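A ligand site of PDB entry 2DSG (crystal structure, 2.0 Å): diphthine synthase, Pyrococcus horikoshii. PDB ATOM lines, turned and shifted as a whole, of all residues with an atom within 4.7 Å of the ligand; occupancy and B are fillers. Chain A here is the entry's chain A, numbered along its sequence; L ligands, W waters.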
ATOM      1  N   LEU A  10       9.915  -2.685 -19.784  1.00  0.00           N
ATOM      2  CA  LEU A  10      10.144  -1.803 -20.927  1.00  0.00           C
ATOM      3  C   LEU A  10       9.395  -0.491 -21.168  1.00  0.00           C
ATOM      4  O   LEU A  10      10.026   0.506 -21.515  1.00  0.00           O
ATOM      5  CB  LEU A  10       9.985  -2.618 -22.213  1.00  0.00           C
ATOM      6  CG  LEU A  10      10.776  -3.921 -22.341  1.00  0.00           C
ATOM      7  CD1 LEU A  10      10.160  -4.787 -23.415  1.00  0.00           C
ATOM      8  CD2 LEU A  10      12.223  -3.623 -22.655  1.00  0.00           C
ATOM      9  N   THR A  36      18.384   5.429 -15.476  1.00  0.00           N
ATOM     10  CA  THR A  36      19.070   4.453 -16.318  1.00  0.00           C
ATOM     11  C   THR A  36      18.335   4.182 -17.638  1.00  0.00           C
ATOM     12  O   THR A  36      18.937   3.716 -18.594  1.00  0.00           O
ATOM     13  CB  THR A  36      19.275   3.097 -15.587  1.00  0.00           C
ATOM     14  OG1 THR A  36      18.008   2.604 -15.114  1.00  0.00           O
ATOM     15  CG2 THR A  36      20.218   3.270 -14.414  1.00  0.00           C
ATOM     16  N   SER A  37      17.041   4.477 -17.672  1.00  0.00           N
ATOM     17  CA  SER A  37      16.281   4.275 -18.894  1.00  0.00           C
ATOM     18  C   SER A  37      14.984   5.077 -18.826  1.00  0.00           C
ATOM     19  O   SER A  37      14.653   5.637 -17.786  1.00  0.00           O
ATOM     20  CB  SER A  37      15.944   2.797 -19.099  1.00  0.00           C
ATOM     21  OG  SER A  37      15.295   2.609 -20.340  1.00  0.00           O
ATOM     22  N   LEU A  38      14.264   5.121 -19.944  1.00  0.00           N
ATOM     23  CA  LEU A  38      13.008   5.855 -20.012  1.00  0.00           C
ATOM     24  C   LEU A  38      11.799   4.948 -20.245  1.00  0.00           C
ATOM     25  O   LEU A  38      11.766   4.176 -21.202  1.00  0.00           O
ATOM     26  CB  LEU A  38      13.069   6.896 -21.138  1.00  0.00           C
ATOM     27  CG  LEU A  38      11.777   7.678 -21.394  1.00  0.00           C
ATOM     28  CD1 LEU A  38      11.448   8.553 -20.188  1.00  0.00           C
ATOM     29  CD2 LEU A  38      11.940   8.537 -22.652  1.00  0.00           C
ATOM     30  N   PRO A  85      13.793   0.792 -14.243  1.00  0.00           N
ATOM     31  CA  PRO A  85      13.148   0.515 -15.522  1.00  0.00           C
ATOM     32  C   PRO A  85      13.768  -0.787 -16.045  1.00  0.00           C
ATOM     33  O   PRO A  85      14.826  -1.191 -15.576  1.00  0.00           O
ATOM     34  CB  PRO A  85      13.542   1.720 -16.379  1.00  0.00           C
ATOM     35  CG  PRO A  85      13.766   2.810 -15.350  1.00  0.00           C
ATOM     36  CD  PRO A  85      14.498   2.085 -14.260  1.00  0.00           C
ATOM     37  N   GLY A  86      13.114  -1.433 -17.019  1.00  0.00           N
ATOM     38  CA  GLY A  86      13.635  -2.669 -17.588  1.00  0.00           C
ATOM     39  C   GLY A  86      14.071  -3.686 -16.541  1.00  0.00           C
ATOM     40  O   GLY A  86      13.350  -3.894 -15.564  1.00  0.00           O
ATOM     41  N   ASP A  87      15.209  -4.324 -16.765  1.00  0.00           N
ATOM     42  CA  ASP A  87      15.762  -5.305 -15.835  1.00  0.00           C
ATOM     43  C   ASP A  87      16.801  -4.515 -15.020  1.00  0.00           C
ATOM     44  O   ASP A  87      17.662  -3.836 -15.598  1.00  0.00           O
ATOM     45  CB  ASP A  87      16.420  -6.452 -16.590  1.00  0.00           C
ATOM     46  CG  ASP A  87      16.948  -7.541 -15.656  1.00  0.00           C
ATOM     47  OD1 ASP A  87      17.900  -7.266 -14.898  1.00  0.00           O
ATOM     48  OD2 ASP A  87      16.408  -8.672 -15.703  1.00  0.00           O
ATOM     49  N   VAL A  90      20.718  -5.004 -16.121  1.00  0.00           N
ATOM     50  CA  VAL A  90      21.121  -4.976 -17.522  1.00  0.00           C
ATOM     51  C   VAL A  90      21.522  -3.554 -17.932  1.00  0.00           C
ATOM     52  O   VAL A  90      20.716  -2.628 -17.882  1.00  0.00           O
ATOM     53  CB  VAL A  90      19.980  -5.456 -18.444  1.00  0.00           C
ATOM     54  CG1 VAL A  90      20.351  -5.224 -19.897  1.00  0.00           C
ATOM     55  CG2 VAL A  90      19.709  -6.931 -18.192  1.00  0.00           C
ATOM     56  N   ALA A  91      22.776  -3.392 -18.342  1.00  0.00           N
ATOM     57  CA  ALA A  91      23.268  -2.094 -18.782  1.00  0.00           C
ATOM     58  C   ALA A  91      23.141  -1.016 -17.717  1.00  0.00           C
ATOM     59  O   ALA A  91      22.826   0.143 -18.011  1.00  0.00           O
ATOM     60  CB  ALA A  91      22.548  -1.655 -20.061  1.00  0.00           C
ATOM     61  N   THR A  92      23.363  -1.406 -16.462  1.00  0.00           N
ATOM     62  CA  THR A  92      23.350  -0.487 -15.331  1.00  0.00           C
ATOM     63  C   THR A  92      24.520  -0.968 -14.500  1.00  0.00           C
ATOM     64  O   THR A  92      25.132  -1.995 -14.825  1.00  0.00           O
ATOM     65  CB  THR A  92      22.066  -0.590 -14.469  1.00  0.00           C
ATOM     66  OG1 THR A  92      22.080  -1.834 -13.745  1.00  0.00           O
ATOM     67  CG2 THR A  92      20.822  -0.514 -15.334  1.00  0.00           C
ATOM     68  N   PRO A 114      11.092  -7.595 -18.292  1.00  0.00           N
ATOM     69  CA  PRO A 114      11.468  -7.514 -19.713  1.00  0.00           C
ATOM     70  C   PRO A 114      12.585  -6.489 -19.910  1.00  0.00           C
ATOM     71  O   PRO A 114      12.528  -5.380 -19.372  1.00  0.00           O
ATOM     72  CB  PRO A 114      10.173  -7.061 -20.391  1.00  0.00           C
ATOM     73  CG  PRO A 114       9.102  -7.588 -19.480  1.00  0.00           C
ATOM     74  CD  PRO A 114       9.653  -7.319 -18.112  1.00  0.00           C
ATOM     75  N   SER A 115      13.602  -6.865 -20.685  1.00  0.00           N
ATOM     76  CA  SER A 115      14.739  -5.999 -20.951  1.00  0.00           C
ATOM     77  C   SER A 115      14.860  -5.711 -22.447  1.00  0.00           C
ATOM     78  O   SER A 115      14.530  -6.560 -23.275  1.00  0.00           O
ATOM     79  CB  SER A 115      16.037  -6.657 -20.466  1.00  0.00           C
ATOM     80  OG  SER A 115      17.176  -5.870 -20.801  1.00  0.00           O
ATOM     81  N   ILE A 116      15.341  -4.516 -22.792  1.00  0.00           N
ATOM     82  CA  ILE A 116      15.515  -4.154 -24.186  1.00  0.00           C
ATOM     83  C   ILE A 116      16.550  -5.096 -24.815  1.00  0.00           C
ATOM     84  O   ILE A 116      16.502  -5.399 -26.010  1.00  0.00           O
ATOM     85  CB  ILE A 116      15.990  -2.674 -24.322  1.00  0.00           C
ATOM     86  CG1 ILE A 116      16.019  -2.252 -25.798  1.00  0.00           C
ATOM     87  CG2 ILE A 116      17.378  -2.500 -23.701  1.00  0.00           C
ATOM     88  CD1 ILE A 116      14.654  -2.265 -26.463  1.00  0.00           C
ATOM     89  N   PHE A 165      22.846   0.740 -27.485  1.00  0.00           N
ATOM     90  CA  PHE A 165      22.032   1.418 -26.492  1.00  0.00           C
ATOM     91  C   PHE A 165      22.269   2.887 -26.806  1.00  0.00           C
ATOM     92  O   PHE A 165      23.382   3.265 -27.163  1.00  0.00           O
ATOM     93  CB  PHE A 165      22.530   1.108 -25.080  1.00  0.00           C
ATOM     94  CG  PHE A 165      22.320  -0.316 -24.645  1.00  0.00           C
ATOM     95  CD1 PHE A 165      21.087  -0.732 -24.150  1.00  0.00           C
ATOM     96  CD2 PHE A 165      23.363  -1.244 -24.720  1.00  0.00           C
ATOM     97  CE1 PHE A 165      20.889  -2.046 -23.724  1.00  0.00           C
ATOM     98  CE2 PHE A 165      23.174  -2.558 -24.299  1.00  0.00           C
ATOM     99  CZ  PHE A 165      21.941  -2.964 -23.803  1.00  0.00           C
ATOM    100  N   LEU A 166      21.242   3.722 -26.678  1.00  0.00           N
ATOM    101  CA  LEU A 166      21.424   5.143 -26.963  1.00  0.00           C
ATOM    102  C   LEU A 166      21.468   5.945 -25.667  1.00  0.00           C
ATOM    103  O   LEU A 166      20.848   5.579 -24.661  1.00  0.00           O
ATOM    104  CB  LEU A 166      20.304   5.624 -27.887  1.00  0.00           C
ATOM    105  CG  LEU A 166      20.198   4.817 -29.204  1.00  0.00           C
ATOM    106  CD1 LEU A 166      19.200   5.482 -30.142  1.00  0.00           C
ATOM    107  CD2 LEU A 166      21.584   4.739 -29.888  1.00  0.00           C
ATOM    108  N   ASP A 167      22.229   7.045 -25.683  1.00  0.00           N
ATOM    109  CA  ASP A 167      22.404   7.872 -24.499  1.00  0.00           C
ATOM    110  C   ASP A 167      21.132   8.477 -23.916  1.00  0.00           C
ATOM    111  O   ASP A 167      20.118   8.635 -24.607  1.00  0.00           O
ATOM    112  CB  ASP A 167      23.408   8.986 -24.777  1.00  0.00           C
ATOM    113  CG  ASP A 167      24.213   9.365 -23.542  1.00  0.00           C
ATOM    114  OD1 ASP A 167      23.890   8.860 -22.440  1.00  0.00           O
ATOM    115  OD2 ASP A 167      25.165  10.167 -23.666  1.00  0.00           O
ATOM    116  N   ILE A 168      21.195   8.807 -22.629  1.00  0.00           N
ATOM    117  CA  ILE A 168      20.080   9.400 -21.912  1.00  0.00           C
ATOM    118  C   ILE A 168      20.597  10.351 -20.829  1.00  0.00           C
ATOM    119  O   ILE A 168      21.527  10.016 -20.083  1.00  0.00           O
ATOM    120  CB  ILE A 168      19.194   8.318 -21.239  1.00  0.00           C
ATOM    121  CG1 ILE A 168      18.158   8.991 -20.324  1.00  0.00           C
ATOM    122  CG2 ILE A 168      20.063   7.353 -20.437  1.00  0.00           C
ATOM    123  CD1 ILE A 168      17.249   8.018 -19.582  1.00  0.00           C
ATOM    124  N   LEU A 206      14.342   0.339 -33.347  1.00  0.00           N
ATOM    125  CA  LEU A 206      13.254  -0.155 -32.514  1.00  0.00           C
ATOM    126  C   LEU A 206      12.962   0.954 -31.525  1.00  0.00           C
ATOM    127  O   LEU A 206      13.831   1.333 -30.741  1.00  0.00           O
ATOM    128  CB  LEU A 206      13.661  -1.423 -31.768  1.00  0.00           C
ATOM    129  CG  LEU A 206      12.600  -1.982 -30.799  1.00  0.00           C
ATOM    130  CD1 LEU A 206      11.299  -2.278 -31.545  1.00  0.00           C
ATOM    131  CD2 LEU A 206      13.133  -3.254 -30.144  1.00  0.00           C
ATOM    132  N   ALA A 207      11.747   1.485 -31.576  1.00  0.00           N
ATOM    133  CA  ALA A 207      11.366   2.552 -30.673  1.00  0.00           C
ATOM    134  C   ALA A 207      10.186   2.153 -29.812  1.00  0.00           C
ATOM    135  O   ALA A 207       9.212   1.581 -30.309  1.00  0.00           O
ATOM    136  CB  ALA A 207      11.014   3.818 -31.472  1.00  0.00           C
ATOM    137  N   ARG A 208      10.291   2.450 -28.521  1.00  0.00           N
ATOM    138  CA  ARG A 208       9.226   2.161 -27.569  1.00  0.00           C
ATOM    139  C   ARG A 208       8.872   0.685 -27.478  1.00  0.00           C
ATOM    140  O   ARG A 208       7.694   0.311 -27.493  1.00  0.00           O
ATOM    141  CB  ARG A 208       7.982   3.003 -27.904  1.00  0.00           C
ATOM    142  CG  ARG A 208       8.262   4.512 -27.965  1.00  0.00           C
ATOM    143  CD  ARG A 208       6.993   5.305 -28.304  1.00  0.00           C
ATOM    144  NE  ARG A 208       6.361   4.774 -29.515  1.00  0.00           N
ATOM    145  CZ  ARG A 208       6.880   4.881 -30.732  1.00  0.00           C
ATOM    146  NH1 ARG A 208       8.039   5.512 -30.911  1.00  0.00           N
ATOM    147  NH2 ARG A 208       6.261   4.335 -31.767  1.00  0.00           N
ATOM    148  N   ALA A 209       9.898  -0.157 -27.382  1.00  0.00           N
ATOM    149  CA  ALA A 209       9.681  -1.592 -27.245  1.00  0.00           C
ATOM    150  C   ALA A 209       8.865  -1.733 -25.961  1.00  0.00           C
ATOM    151  O   ALA A 209       9.061  -0.970 -25.024  1.00  0.00           O
ATOM    152  CB  ALA A 209      11.028  -2.323 -27.103  1.00  0.00           C
ATOM    153  N   PRO A 233      11.953   6.003 -25.768  1.00  0.00           N
ATOM    154  CA  PRO A 233      13.345   5.673 -26.094  1.00  0.00           C
ATOM    155  C   PRO A 233      13.487   4.943 -27.414  1.00  0.00           C
ATOM    156  O   PRO A 233      12.551   4.298 -27.887  1.00  0.00           O
ATOM    157  CB  PRO A 233      13.776   4.823 -24.908  1.00  0.00           C
ATOM    158  CG  PRO A 233      12.516   4.034 -24.636  1.00  0.00           C
ATOM    159  CD  PRO A 233      11.419   5.081 -24.748  1.00  0.00           C
ATOM    160  N   HIS A 234      14.686   5.032 -27.988  1.00  0.00           N
ATOM    161  CA  HIS A 234      15.003   4.380 -29.252  1.00  0.00           C
ATOM    162  C   HIS A 234      16.245   3.532 -29.035  1.00  0.00           C
ATOM    163  O   HIS A 234      17.043   3.792 -28.145  1.00  0.00           O
ATOM    164  CB  HIS A 234      15.351   5.395 -30.348  1.00  0.00           C
ATOM    165  CG  HIS A 234      14.220   6.243 -30.811  1.00  0.00           C
ATOM    166  ND1 HIS A 234      14.360   7.196 -31.799  1.00  0.00           N
ATOM    167  CD2 HIS A 234      12.909   6.286 -30.434  1.00  0.00           C
ATOM    168  CE1 HIS A 234      13.192   7.779 -32.015  1.00  0.00           C
ATOM    169  NE2 HIS A 234      12.301   7.244 -31.194  1.00  0.00           N
ATOM    170  N   ILE A 235      16.413   2.526 -29.886  1.00  0.00           N
ATOM    171  CA  ILE A 235      17.592   1.686 -29.837  1.00  0.00           C
ATOM    172  C   ILE A 235      17.971   1.517 -31.304  1.00  0.00           C
ATOM    173  O   ILE A 235      17.107   1.461 -32.169  1.00  0.00           O
ATOM    174  CB  ILE A 235      17.300   0.301 -29.198  1.00  0.00           C
ATOM    175  CG1 ILE A 235      18.584  -0.279 -28.619  1.00  0.00           C
ATOM    176  CG2 ILE A 235      16.740  -0.659 -30.224  1.00  0.00           C
ATOM    177  CD1 ILE A 235      18.744  -0.041 -27.149  1.00  0.00           C
HETATM  178  N1  LIG L   1      18.160  -1.999 -17.671  1.00  0.00           N
HETATM  179  C1  LIG L   1      17.481  -1.453 -18.939  1.00  0.00           C
HETATM  180  C2  LIG L   1      18.360  -0.722 -19.927  1.00  0.00           C
HETATM  181  C3  LIG L   1      19.145   0.483 -19.466  1.00  0.00           C
HETATM  182  S1  LIG L   1      19.938   1.214 -20.968  1.00  0.00           S
HETATM  183  C4  LIG L   1      16.768  -2.675 -19.631  1.00  0.00           C
HETATM  184  O1  LIG L   1      16.863  -3.798 -19.103  1.00  0.00           O
HETATM  185  O2  LIG L   1      16.108  -2.425 -20.729  1.00  0.00           O
HETATM  186  C5  LIG L   1      18.716   2.378 -21.423  1.00  0.00           C
HETATM  187  C6  LIG L   1      18.697   2.525 -22.991  1.00  0.00           C
HETATM  188  O3  LIG L   1      18.217   1.276 -23.548  1.00  0.00           O
HETATM  189  C7  LIG L   1      17.816   3.593 -23.526  1.00  0.00           C
HETATM  190  O4  LIG L   1      18.500   4.839 -23.592  1.00  0.00           O
HETATM  191  C8  LIG L   1      17.400   3.015 -24.896  1.00  0.00           C
HETATM  192  O5  LIG L   1      18.380   3.280 -25.903  1.00  0.00           O
HETATM  193  C9  LIG L   1      17.193   1.515 -24.616  1.00  0.00           C
HETATM  194  N2  LIG L   1      15.961   1.181 -24.181  1.00  0.00           N
HETATM  195  C10 LIG L   1      15.406   0.856 -22.951  1.00  0.00           C
HETATM  196  N3  LIG L   1      14.132   0.598 -22.978  1.00  0.00           N
HETATM  197  C11 LIG L   1      13.760   0.759 -24.349  1.00  0.00           C
HETATM  198  C12 LIG L   1      12.496   0.609 -25.015  1.00  0.00           C
HETATM  199  N4  LIG L   1      11.354   0.265 -24.400  1.00  0.00           N
HETATM  200  N5  LIG L   1      12.528   0.848 -26.373  1.00  0.00           N
HETATM  201  C13 LIG L   1      13.650   1.195 -27.044  1.00  0.00           C
HETATM  202  N6  LIG L   1      14.880   1.349 -26.440  1.00  0.00           N
HETATM  203  C14 LIG L   1      14.853   1.110 -25.094  1.00  0.00           C
HETATM  204  O   HOH W   1      17.314   0.308 -16.477  1.00  0.00           O
HETATM  205  O   HOH W   2      17.423   7.245 -24.296  1.00  0.00           O
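S1 of the ligand sits close to O of Thr 36 (3.6 Å).
Ser 37 touches the ligand.
Gly 86 touches the ligand (CA to C4, 3.7 Å).
Ala 91 touches the ligand.
Thr 92 touches the ligand (CG2 to N1, 3.8 Å).
Phe 165 touches the ligand (CD1 to O3, 3.6 Å).
Leu 206 touches the ligand.
O of Pro 233 touches C13 of the ligand, at 3.4 Å.
CD1 of Ile 235 touches C9 of the ligand, at 3.4 Å.
Hydrophobic or aromatic side chains within 4 Å of the ligand: Leu 10, Val 90, Ala 91, Ile 116, Phe 165, Leu 166, Ala 209, Pro 233 and Ile 235.
Water W2 bridges O4 of the ligand (2.7 Å) and O of Asp 167 (3.0 Å).
Water W1 lies within hydrogen-bond range of N1 of the ligand, OG1 of Thr 36 and O of Pro 85.
O of Val 90 sits at hydrogen-bond distance from N1 of the ligand, at 2.6 Å.
The backbone carbonyl oxygen (O) of His 234 is in hydrogen-bond range of an oxygen (O5) of the ligand (2.7 Å).
N5 of the ligand sits at hydrogen-bond distance from N of Ala 209, at 3.0 Å.
The backbone carbonyl oxygen (O) of Ala 209 lies within hydrogen-bond range of a nitrogen (N4) of the ligand, at 2.7 Å.
An oxygen (O5) of the ligand sits at hydrogen-bond distance from the backbone NH (N) of Leu 166, 3.0 Å away.
An oxygen (O4) of the ligand sits at hydrogen-bond distance from the backbone carbonyl oxygen of Leu 166.
The side-chain hydroxyl of Ser 115 lies within hydrogen-bond range of an oxygen (O1) of the ligand, at 2.7 Å.
The backbone NH (N) of Asp 87 lies within hydrogen-bond range of an oxygen (O1) of the ligand (2.9 Å).
The backbone carbonyl oxygen of Asp 87 sits at hydrogen-bond distance from a nitrogen (N1) of the ligand (2.8 Å).
N of Ile 116 sits at hydrogen-bond distance from O2 of the ligand (3.0 Å).
A nitrogen (N4) of the ligand is in hydrogen-bond range of the backbone carbonyl oxygen (O) of Leu 10, at 3.2 Å.
A nitrogen (N5) of the ligand lies within hydrogen-bond range of the backbone NH of Arg 208, 3.5 Å away.
N of Ile 235 lies within hydrogen-bond range of O of Leu 206 (3.0 Å).
The backbone carbonyl oxygen (O) of Pro 233 is in hydrogen-bond range of the backbone NH (N) of Arg 208 (3.0 Å).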
